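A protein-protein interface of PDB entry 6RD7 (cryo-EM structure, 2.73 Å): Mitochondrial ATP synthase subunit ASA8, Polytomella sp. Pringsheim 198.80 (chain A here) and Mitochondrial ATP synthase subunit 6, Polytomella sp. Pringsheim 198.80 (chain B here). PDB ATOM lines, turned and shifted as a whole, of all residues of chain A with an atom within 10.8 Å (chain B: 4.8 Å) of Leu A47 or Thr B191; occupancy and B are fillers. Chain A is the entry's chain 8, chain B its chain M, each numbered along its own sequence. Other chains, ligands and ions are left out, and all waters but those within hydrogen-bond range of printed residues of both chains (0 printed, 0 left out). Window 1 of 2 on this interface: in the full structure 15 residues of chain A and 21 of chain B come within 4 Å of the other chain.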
ATOM      1  N   TYR A  35       4.105  18.849   1.841  1.00  0.00           N
ATOM      2  CA  TYR A  35       3.660  17.616   2.477  1.00  0.00           C
ATOM      3  C   TYR A  35       4.625  16.472   2.209  1.00  0.00           C
ATOM      4  O   TYR A  35       4.855  15.629   3.082  1.00  0.00           O
ATOM      5  CB  TYR A  35       2.263  17.255   1.987  1.00  0.00           C
ATOM      6  CG  TYR A  35       1.836  15.876   2.395  1.00  0.00           C
ATOM      7  CD1 TYR A  35       1.679  15.555   3.732  1.00  0.00           C
ATOM      8  CD2 TYR A  35       1.602  14.889   1.449  1.00  0.00           C
ATOM      9  CE1 TYR A  35       1.301  14.303   4.117  1.00  0.00           C
ATOM     10  CE2 TYR A  35       1.218  13.627   1.827  1.00  0.00           C
ATOM     11  CZ  TYR A  35       1.067  13.342   3.164  1.00  0.00           C
ATOM     12  OH  TYR A  35       0.685  12.086   3.556  1.00  0.00           O
ATOM     13  N   LYS A  39       6.231  15.748   5.722  1.00  0.00           N
ATOM     14  CA  LYS A  39       5.525  14.677   6.415  1.00  0.00           C
ATOM     15  C   LYS A  39       5.522  13.354   5.671  1.00  0.00           C
ATOM     16  O   LYS A  39       5.636  12.307   6.311  1.00  0.00           O
ATOM     17  CB  LYS A  39       4.079  15.089   6.723  1.00  0.00           C
ATOM     18  CG  LYS A  39       3.422  14.189   7.758  1.00  0.00           C
ATOM     19  CD  LYS A  39       2.068  14.677   8.178  1.00  0.00           C
ATOM     20  CE  LYS A  39       2.021  14.904   9.668  1.00  0.00           C
ATOM     21  NZ  LYS A  39       0.732  15.505  10.085  1.00  0.00           N
ATOM     22  N   LEU A  40       5.399  13.356   4.342  1.00  0.00           N
ATOM     23  CA  LEU A  40       5.175  12.096   3.635  1.00  0.00           C
ATOM     24  C   LEU A  40       6.423  11.226   3.627  1.00  0.00           C
ATOM     25  O   LEU A  40       6.365  10.059   4.024  1.00  0.00           O
ATOM     26  CB  LEU A  40       4.696  12.353   2.212  1.00  0.00           C
ATOM     27  CG  LEU A  40       4.522  11.104   1.355  1.00  0.00           C
ATOM     28  CD1 LEU A  40       3.386  10.256   1.881  1.00  0.00           C
ATOM     29  CD2 LEU A  40       4.279  11.483  -0.087  1.00  0.00           C
ATOM     30  N   ILE A  41       7.561  11.779   3.220  1.00  0.00           N
ATOM     31  CA  ILE A  41       8.823  11.049   3.326  1.00  0.00           C
ATOM     32  C   ILE A  41       9.189  10.796   4.791  1.00  0.00           C
ATOM     33  O   ILE A  41       9.151   9.619   5.178  1.00  0.00           O
ATOM     34  CB  ILE A  41       9.957  11.743   2.549  1.00  0.00           C
ATOM     35  CG1 ILE A  41       9.633  11.807   1.054  1.00  0.00           C
ATOM     36  CG2 ILE A  41      11.257  11.012   2.760  1.00  0.00           C
ATOM     37  CD1 ILE A  41       9.202  10.498   0.452  1.00  0.00           C
ATOM     38  N   PRO A  42       9.440  11.800   5.665  1.00  0.00           N
ATOM     39  CA  PRO A  42      10.078  11.477   6.955  1.00  0.00           C
ATOM     40  C   PRO A  42       9.191  10.743   7.947  1.00  0.00           C
ATOM     41  O   PRO A  42       9.702  10.232   8.950  1.00  0.00           O
ATOM     42  CB  PRO A  42      10.474  12.857   7.503  1.00  0.00           C
ATOM     43  CG  PRO A  42      10.186  13.825   6.422  1.00  0.00           C
ATOM     44  CD  PRO A  42       9.073  13.228   5.676  1.00  0.00           C
ATOM     45  N   ARG A  43       7.890  10.668   7.710  1.00  0.00           N
ATOM     46  CA  ARG A  43       7.014   9.909   8.586  1.00  0.00           C
ATOM     47  C   ARG A  43       6.374   8.703   7.925  1.00  0.00           C
ATOM     48  O   ARG A  43       6.055   7.745   8.627  1.00  0.00           O
ATOM     49  CB  ARG A  43       5.904  10.803   9.155  1.00  0.00           C
ATOM     50  CG  ARG A  43       6.402  11.986   9.954  1.00  0.00           C
ATOM     51  CD  ARG A  43       6.925  11.554  11.302  1.00  0.00           C
ATOM     52  NE  ARG A  43       5.844  11.196  12.208  1.00  0.00           N
ATOM     53  CZ  ARG A  43       6.017  10.535  13.345  1.00  0.00           C
ATOM     54  NH1 ARG A  43       7.230  10.158  13.707  1.00  0.00           N
ATOM     55  NH2 ARG A  43       4.980  10.249  14.114  1.00  0.00           N
ATOM     56  N   HIS A  44       6.183   8.708   6.606  1.00  0.00           N
ATOM     57  CA  HIS A  44       5.461   7.646   5.923  1.00  0.00           C
ATOM     58  C   HIS A  44       6.338   6.910   4.920  1.00  0.00           C
ATOM     59  O   HIS A  44       5.821   6.195   4.052  1.00  0.00           O
ATOM     60  CB  HIS A  44       4.223   8.197   5.222  1.00  0.00           C
ATOM     61  CG  HIS A  44       3.320   8.987   6.114  1.00  0.00           C
ATOM     62  ND1 HIS A  44       2.925   8.545   7.355  1.00  0.00           N
ATOM     63  CD2 HIS A  44       2.730  10.190   5.940  1.00  0.00           C
ATOM     64  CE1 HIS A  44       2.132   9.441   7.909  1.00  0.00           C
ATOM     65  NE2 HIS A  44       1.998  10.450   7.071  1.00  0.00           N
ATOM     66  N   TRP A  45       7.662   7.059   5.014  1.00  0.00           N
ATOM     67  CA  TRP A  45       8.505   6.305   4.100  1.00  0.00           C
ATOM     68  C   TRP A  45       8.525   4.816   4.408  1.00  0.00           C
ATOM     69  O   TRP A  45       8.835   4.031   3.512  1.00  0.00           O
ATOM     70  CB  TRP A  45       9.924   6.878   4.090  1.00  0.00           C
ATOM     71  CG  TRP A  45      10.763   6.557   5.280  1.00  0.00           C
ATOM     72  CD1 TRP A  45      10.896   7.299   6.409  1.00  0.00           C
ATOM     73  CD2 TRP A  45      11.622   5.426   5.440  1.00  0.00           C
ATOM     74  NE1 TRP A  45      11.769   6.693   7.272  1.00  0.00           N
ATOM     75  CE2 TRP A  45      12.228   5.538   6.700  1.00  0.00           C
ATOM     76  CE3 TRP A  45      11.925   4.319   4.643  1.00  0.00           C
ATOM     77  CZ2 TRP A  45      13.123   4.594   7.179  1.00  0.00           C
ATOM     78  CZ3 TRP A  45      12.807   3.384   5.122  1.00  0.00           C
ATOM     79  CH2 TRP A  45      13.397   3.524   6.379  1.00  0.00           C
ATOM     80  N   TYR A  46       8.150   4.413   5.624  1.00  0.00           N
ATOM     81  CA  TYR A  46       7.971   2.996   5.925  1.00  0.00           C
ATOM     82  C   TYR A  46       6.818   2.405   5.122  1.00  0.00           C
ATOM     83  O   TYR A  46       6.957   1.331   4.527  1.00  0.00           O
ATOM     84  CB  TYR A  46       7.732   2.802   7.420  1.00  0.00           C
ATOM     85  CG  TYR A  46       8.663   3.568   8.329  1.00  0.00           C
ATOM     86  CD1 TYR A  46       9.891   3.041   8.695  1.00  0.00           C
ATOM     87  CD2 TYR A  46       8.300   4.802   8.848  1.00  0.00           C
ATOM     88  CE1 TYR A  46      10.737   3.729   9.536  1.00  0.00           C
ATOM     89  CE2 TYR A  46       9.140   5.496   9.687  1.00  0.00           C
ATOM     90  CZ  TYR A  46      10.357   4.955  10.027  1.00  0.00           C
ATOM     91  OH  TYR A  46      11.201   5.644  10.865  1.00  0.00           O
ATOM     92  N   LEU A  47       5.674   3.103   5.083  1.00  0.00           N
ATOM     93  CA  LEU A  47       4.548   2.666   4.258  1.00  0.00           C
ATOM     94  C   LEU A  47       4.898   2.684   2.783  1.00  0.00           C
ATOM     95  O   LEU A  47       4.493   1.791   2.031  1.00  0.00           O
ATOM     96  CB  LEU A  47       3.327   3.551   4.455  1.00  0.00           C
ATOM     97  CG  LEU A  47       2.423   3.637   5.659  1.00  0.00           C
ATOM     98  CD1 LEU A  47       1.343   4.597   5.231  1.00  0.00           C
ATOM     99  CD2 LEU A  47       1.843   2.295   5.997  1.00  0.00           C
ATOM    100  N   LEU A  48       5.594   3.734   2.343  1.00  0.00           N
ATOM    101  CA  LEU A  48       5.967   3.841   0.937  1.00  0.00           C
ATOM    102  C   LEU A  48       6.909   2.717   0.523  1.00  0.00           C
ATOM    103  O   LEU A  48       6.737   2.127  -0.551  1.00  0.00           O
ATOM    104  CB  LEU A  48       6.595   5.208   0.675  1.00  0.00           C
ATOM    105  CG  LEU A  48       5.710   6.317   0.099  1.00  0.00           C
ATOM    106  CD1 LEU A  48       4.490   6.592   0.961  1.00  0.00           C
ATOM    107  CD2 LEU A  48       6.527   7.583  -0.067  1.00  0.00           C
ATOM    108  N   GLY A  49       7.855   2.361   1.392  1.00  0.00           N
ATOM    109  CA  GLY A  49       8.709   1.221   1.124  1.00  0.00           C
ATOM    110  C   GLY A  49       7.974  -0.103   1.194  1.00  0.00           C
ATOM    111  O   GLY A  49       8.321  -1.043   0.481  1.00  0.00           O
ATOM    112  N   GLY A  50       6.945  -0.195   2.039  1.00  0.00           N
ATOM    113  CA  GLY A  50       6.158  -1.418   2.091  1.00  0.00           C
ATOM    114  C   GLY A  50       5.327  -1.638   0.841  1.00  0.00           C
ATOM    115  O   GLY A  50       5.249  -2.758   0.322  1.00  0.00           O
ATOM    116  N   PHE A  51       4.707  -0.568   0.336  1.00  0.00           N
ATOM    117  CA  PHE A  51       3.997  -0.637  -0.938  1.00  0.00           C
ATOM    118  C   PHE A  51       4.953  -0.940  -2.085  1.00  0.00           C
ATOM    119  O   PHE A  51       4.617  -1.707  -2.995  1.00  0.00           O
ATOM    120  CB  PHE A  51       3.258   0.674  -1.199  1.00  0.00           C
ATOM    121  CG  PHE A  51       2.068   0.885  -0.316  1.00  0.00           C
ATOM    122  CD1 PHE A  51       1.173  -0.140  -0.090  1.00  0.00           C
ATOM    123  CD2 PHE A  51       1.837   2.112   0.278  1.00  0.00           C
ATOM    124  CE1 PHE A  51       0.080   0.045   0.723  1.00  0.00           C
ATOM    125  CE2 PHE A  51       0.742   2.304   1.090  1.00  0.00           C
ATOM    126  CZ  PHE A  51      -0.133   1.266   1.312  1.00  0.00           C
ATOM    127  N   THR A  52       6.158  -0.358  -2.040  1.00  0.00           N
ATOM    128  CA  THR A  52       7.184  -0.642  -3.039  1.00  0.00           C
ATOM    129  C   THR A  52       7.608  -2.107  -3.002  1.00  0.00           C
ATOM    130  O   THR A  52       7.755  -2.746  -4.054  1.00  0.00           O
ATOM    131  CB  THR A  52       8.378   0.283  -2.800  1.00  0.00           C
ATOM    132  OG1 THR A  52       7.992   1.634  -3.072  1.00  0.00           O
ATOM    133  CG2 THR A  52       9.555  -0.077  -3.687  1.00  0.00           C
ATOM    134  N   PHE A  53       7.761  -2.663  -1.796  1.00  0.00           N
ATOM    135  CA  PHE A  53       8.127  -4.067  -1.645  1.00  0.00           C
ATOM    136  C   PHE A  53       7.043  -4.985  -2.178  1.00  0.00           C
ATOM    137  O   PHE A  53       7.342  -5.995  -2.819  1.00  0.00           O
ATOM    138  CB  PHE A  53       8.405  -4.392  -0.177  1.00  0.00           C
ATOM    139  CG  PHE A  53       8.670  -5.851   0.082  1.00  0.00           C
ATOM    140  CD1 PHE A  53       9.904  -6.400  -0.209  1.00  0.00           C
ATOM    141  CD2 PHE A  53       7.687  -6.674   0.617  1.00  0.00           C
ATOM    142  CE1 PHE A  53      10.151  -7.736   0.026  1.00  0.00           C
ATOM    143  CE2 PHE A  53       7.929  -8.005   0.848  1.00  0.00           C
ATOM    144  CZ  PHE A  53       9.162  -8.536   0.555  1.00  0.00           C
ATOM    145  N   THR A  54       5.779  -4.655  -1.919  1.00  0.00           N
ATOM    146  CA  THR A  54       4.702  -5.518  -2.387  1.00  0.00           C
ATOM    147  C   THR A  54       4.552  -5.456  -3.899  1.00  0.00           C
ATOM    148  O   THR A  54       4.307  -6.483  -4.541  1.00  0.00           O
ATOM    149  CB  THR A  54       3.396  -5.146  -1.710  1.00  0.00           C
ATOM    150  OG1 THR A  54       3.639  -4.956  -0.317  1.00  0.00           O
ATOM    151  CG2 THR A  54       2.396  -6.253  -1.880  1.00  0.00           C
ATOM    152  N   ILE A  55       4.729  -4.272  -4.490  1.00  0.00           N
ATOM    153  CA  ILE A  55       4.647  -4.149  -5.944  1.00  0.00           C
ATOM    154  C   ILE A  55       5.806  -4.892  -6.611  1.00  0.00           C
ATOM    155  O   ILE A  55       5.613  -5.604  -7.606  1.00  0.00           O
ATOM    156  CB  ILE A  55       4.589  -2.662  -6.338  1.00  0.00           C
ATOM    157  CG1 ILE A  55       3.232  -2.081  -5.948  1.00  0.00           C
ATOM    158  CG2 ILE A  55       4.800  -2.467  -7.821  1.00  0.00           C
ATOM    159  CD1 ILE A  55       3.212  -0.579  -5.853  1.00  0.00           C
ATOM    160  N   THR A  56       7.001  -4.815  -6.019  1.00  0.00           N
ATOM    161  CA  THR A  56       8.157  -5.541  -6.542  1.00  0.00           C
ATOM    162  C   THR A  56       7.974  -7.054  -6.421  1.00  0.00           C
ATOM    163  O   THR A  56       8.223  -7.801  -7.380  1.00  0.00           O
ATOM    164  CB  THR A  56       9.415  -5.082  -5.807  1.00  0.00           C
ATOM    165  OG1 THR A  56       9.639  -3.695  -6.076  1.00  0.00           O
ATOM    166  CG2 THR A  56      10.626  -5.872  -6.250  1.00  0.00           C
ATOM    167  N   TRP B 151      -1.559   5.390  10.020  1.00  0.00           N
ATOM    168  CA  TRP B 151      -1.514   4.221   9.149  1.00  0.00           C
ATOM    169  C   TRP B 151      -2.695   3.300   9.409  1.00  0.00           C
ATOM    170  O   TRP B 151      -3.308   2.784   8.469  1.00  0.00           O
ATOM    171  CB  TRP B 151      -0.209   3.452   9.348  1.00  0.00           C
ATOM    172  CG  TRP B 151       1.049   4.218   9.122  1.00  0.00           C
ATOM    173  CD1 TRP B 151       1.176   5.438   8.545  1.00  0.00           C
ATOM    174  CD2 TRP B 151       2.370   3.804   9.471  1.00  0.00           C
ATOM    175  NE1 TRP B 151       2.486   5.818   8.522  1.00  0.00           N
ATOM    176  CE2 TRP B 151       3.243   4.830   9.085  1.00  0.00           C
ATOM    177  CE3 TRP B 151       2.895   2.666  10.078  1.00  0.00           C
ATOM    178  CZ2 TRP B 151       4.611   4.752   9.278  1.00  0.00           C
ATOM    179  CZ3 TRP B 151       4.247   2.592  10.268  1.00  0.00           C
ATOM    180  CH2 TRP B 151       5.093   3.627   9.873  1.00  0.00           C
ATOM    181  N   PHE B 155      -5.656   2.373   6.769  1.00  0.00           N
ATOM    182  CA  PHE B 155      -6.018   1.010   6.397  1.00  0.00           C
ATOM    183  C   PHE B 155      -7.443   0.674   6.814  1.00  0.00           C
ATOM    184  O   PHE B 155      -8.157  -0.006   6.070  1.00  0.00           O
ATOM    185  CB  PHE B 155      -5.017   0.020   6.986  1.00  0.00           C
ATOM    186  CG  PHE B 155      -3.762  -0.101   6.176  1.00  0.00           C
ATOM    187  CD1 PHE B 155      -3.801  -0.633   4.901  1.00  0.00           C
ATOM    188  CD2 PHE B 155      -2.551   0.343   6.672  1.00  0.00           C
ATOM    189  CE1 PHE B 155      -2.652  -0.733   4.142  1.00  0.00           C
ATOM    190  CE2 PHE B 155      -1.404   0.256   5.918  1.00  0.00           C
ATOM    191  CZ  PHE B 155      -1.454  -0.285   4.651  1.00  0.00           C
ATOM    192  N   SER B 187       1.909  -5.423   2.417  1.00  0.00           N
ATOM    193  CA  SER B 187       2.418  -4.070   2.599  1.00  0.00           C
ATOM    194  C   SER B 187       2.484  -3.677   4.066  1.00  0.00           C
ATOM    195  O   SER B 187       3.420  -2.986   4.478  1.00  0.00           O
ATOM    196  CB  SER B 187       1.550  -3.088   1.829  1.00  0.00           C
ATOM    197  OG  SER B 187       1.648  -3.321   0.441  1.00  0.00           O
ATOM    198  N   VAL B 188       1.508  -4.113   4.872  1.00  0.00           N
ATOM    199  CA  VAL B 188       1.566  -3.840   6.309  1.00  0.00           C
ATOM    200  C   VAL B 188       2.728  -4.586   6.951  1.00  0.00           C
ATOM    201  O   VAL B 188       3.481  -4.018   7.758  1.00  0.00           O
ATOM    202  CB  VAL B 188       0.230  -4.195   6.986  1.00  0.00           C
ATOM    203  CG1 VAL B 188       0.366  -4.125   8.487  1.00  0.00           C
ATOM    204  CG2 VAL B 188      -0.831  -3.246   6.563  1.00  0.00           C
ATOM    205  N   TRP B 189       2.907  -5.860   6.582  1.00  0.00           N
ATOM    206  CA  TRP B 189       4.021  -6.639   7.114  1.00  0.00           C
ATOM    207  C   TRP B 189       5.361  -6.061   6.685  1.00  0.00           C
ATOM    208  O   TRP B 189       6.314  -6.033   7.470  1.00  0.00           O
ATOM    209  CB  TRP B 189       3.901  -8.089   6.664  1.00  0.00           C
ATOM    210  CG  TRP B 189       5.070  -8.946   7.029  1.00  0.00           C
ATOM    211  CD1 TRP B 189       5.237  -9.646   8.178  1.00  0.00           C
ATOM    212  CD2 TRP B 189       6.229  -9.204   6.229  1.00  0.00           C
ATOM    213  NE1 TRP B 189       6.429 -10.321   8.152  1.00  0.00           N
ATOM    214  CE2 TRP B 189       7.058 -10.065   6.964  1.00  0.00           C
ATOM    215  CE3 TRP B 189       6.646  -8.786   4.963  1.00  0.00           C
ATOM    216  CZ2 TRP B 189       8.277 -10.517   6.479  1.00  0.00           C
ATOM    217  CZ3 TRP B 189       7.855  -9.232   4.486  1.00  0.00           C
ATOM    218  CH2 TRP B 189       8.658 -10.089   5.240  1.00  0.00           C
ATOM    219  N   ALA B 190       5.442  -5.559   5.455  1.00  0.00           N
ATOM    220  CA  ALA B 190       6.680  -4.966   4.979  1.00  0.00           C
ATOM    221  C   ALA B 190       6.941  -3.623   5.640  1.00  0.00           C
ATOM    222  O   ALA B 190       8.093  -3.257   5.865  1.00  0.00           O
ATOM    223  CB  ALA B 190       6.634  -4.814   3.466  1.00  0.00           C
ATOM    224  N   THR B 191       5.881  -2.881   5.968  1.00  0.00           N
ATOM    225  CA  THR B 191       6.033  -1.632   6.704  1.00  0.00           C
ATOM    226  C   THR B 191       6.574  -1.882   8.106  1.00  0.00           C
ATOM    227  O   THR B 191       7.500  -1.193   8.555  1.00  0.00           O
ATOM    228  CB  THR B 191       4.689  -0.914   6.771  1.00  0.00           C
ATOM    229  OG1 THR B 191       4.192  -0.716   5.445  1.00  0.00           O
ATOM    230  CG2 THR B 191       4.827   0.417   7.447  1.00  0.00           C
ATOM    231  N   ALA B 192       6.026  -2.886   8.795  1.00  0.00           N
ATOM    232  CA  ALA B 192       6.521  -3.248  10.121  1.00  0.00           C
ATOM    233  C   ALA B 192       7.950  -3.773  10.055  1.00  0.00           C
ATOM    234  O   ALA B 192       8.783  -3.444  10.909  1.00  0.00           O
ATOM    235  CB  ALA B 192       5.598  -4.281  10.759  1.00  0.00           C
ATOM    236  N   THR B 193       8.265  -4.549   9.015  1.00  0.00           N
ATOM    237  CA  THR B 193       9.611  -5.087   8.860  1.00  0.00           C
ATOM    238  C   THR B 193      10.617  -3.987   8.541  1.00  0.00           C
ATOM    239  O   THR B 193      11.726  -3.986   9.076  1.00  0.00           O
ATOM    240  CB  THR B 193       9.605  -6.161   7.772  1.00  0.00           C
ATOM    241  OG1 THR B 193       8.681  -7.189   8.141  1.00  0.00           O
ATOM    242  CG2 THR B 193      10.975  -6.780   7.598  1.00  0.00           C
ATOM    243  N   ILE B 194      10.230  -3.019   7.708  1.00  0.00           N
ATOM    244  CA  ILE B 194      11.122  -1.921   7.345  1.00  0.00           C
ATOM    245  C   ILE B 194      11.354  -1.006   8.542  1.00  0.00           C
ATOM    246  O   ILE B 194      12.474  -0.528   8.765  1.00  0.00           O
ATOM    247  CB  ILE B 194      10.550  -1.171   6.125  1.00  0.00           C
ATOM    248  CG1 ILE B 194      10.901  -1.922   4.846  1.00  0.00           C
ATOM    249  CG2 ILE B 194      11.065   0.247   6.008  1.00  0.00           C
ATOM    250  CD1 ILE B 194      10.022  -1.573   3.691  1.00  0.00           C
ATOM    251  N   LEU B 195      10.322  -0.806   9.368  1.00  0.00           N
ATOM    252  CA  LEU B 195      10.492  -0.040  10.600  1.00  0.00           C
ATOM    253  C   LEU B 195      11.441  -0.747  11.565  1.00  0.00           C
ATOM    254  O   LEU B 195      12.355  -0.123  12.123  1.00  0.00           O
ATOM    255  CB  LEU B 195       9.131   0.200  11.250  1.00  0.00           C
ATOM    256  CG  LEU B 195       9.128   0.829  12.640  1.00  0.00           C
ATOM    257  CD1 LEU B 195       9.318   2.320  12.559  1.00  0.00           C
ATOM    258  CD2 LEU B 195       7.841   0.508  13.343  1.00  0.00           C
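OG of Ser B187 is in hydrogen-bond range of OG1 of Thr A54, 2.7 Å away. A ring nitrogen (ND1) of His A44 is in hydrogen-bond range of the indole nitrogen (NE1) of Trp B151.
OG1 of Thr A54 lies within hydrogen-bond range of O of Gly A50, at 2.8 Å. N of Trp A45 sits at hydrogen-bond distance from O of Leu A40. The backbone carbonyl oxygen (O) of Ser B187 sits at hydrogen-bond distance from the side-chain hydroxyl (OG1) of Thr B191, 2.6 Å away. The backbone carbonyl oxygen (O) of Trp B189 lies within hydrogen-bond range of the side-chain hydroxyl (OG1) of Thr B193 (2.7 Å).
Among the printed residues, pairs that only touch across the chains: Phe A51 with Ser B187 (3.3 Å), Arg A43 with Trp B151 (3.4 Å), Leu A47 with Trp B151 (3.4 Å), Gly A49 with Ile B194 (3.5 Å), Tyr A46 with Thr B191 (3.6 Å), Phe A53 with Ala B190 (3.6 Å), Tyr A46 with Trp B151 (3.6 Å), Leu A47 with Thr B191 (3.6 Å), Tyr A46 with Leu B195 (3.6 Å), Gly A50 with Ser B187 (3.6 Å), Gly A50 with Ala B190 (3.7 Å), Trp A45 with Ile B194 (3.7 Å), Gly A50 with Ile B194 (3.8 Å), Leu A47 with Phe B155 (3.8 Å), Phe A53 with Trp B189 (3.8 Å), Phe A51 with Phe B155 (3.9 Å) and Gly A50 with Thr B191 (3.95 Å).
Of chain B, only Trp B151, Phe B155 and Thr B191 come within 4 Å of Leu A47. Of the printed residues of chain A, Thr B191 touches Tyr A46, Leu A47 and Gly A50. Of the printed residues of chain A, Trp B151 touches Arg A43 (3.4 Å), His A44 (3.0 Å), Tyr A46 (3.6 Å) and Leu A47 (3.4 Å). Of chain A, only Gly A50 (3.6 Å), Phe A51 (3.3 Å) and Thr A54 (2.7 Å) come within 4 Å of Ser B187. No residue of chain A comes within 4 Å of Val B188. Ala B190 touches two residues of chain A. No residue of chain A comes within 4 Å of Ala B192. No residue of chain A comes within 4 Å of Thr B193. Of chain A, only Trp A45, Gly A49 and Gly A50 come within 4 Å of Ile B194. Of the printed residues of chain A, Trp B189 touches Phe A53 (3.8 Å). Of the printed residues of chain B, Gly A49 touches Ile B194. Tyr A35 touches none of the printed residues of chain B. Thr A56 touches none of the printed residues of chain B. The nearest printed residue of chain B that does not touch Leu A47 is Ser B187 (5.5 Å). The nearest residue of chain A that does not touch Thr B191 is Phe A51 (5.1 Å).
Hydrophobic or aromatic side chains of chain A that line the printed part of chain B: His A44, Trp A45, Tyr A46, Leu A47, Phe A51 and Phe A53. Hydrophobic or aromatic side chains of chain B within 4 Å of the printed part of chain A: Trp B151, Phe B155, Trp B189, Ala B190, Ile B194 and Leu B195. Among the printed residues, no Asp or Glu carboxylate lies within 4 Å of a Lys or Arg side-chain nitrogen of the other chain.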
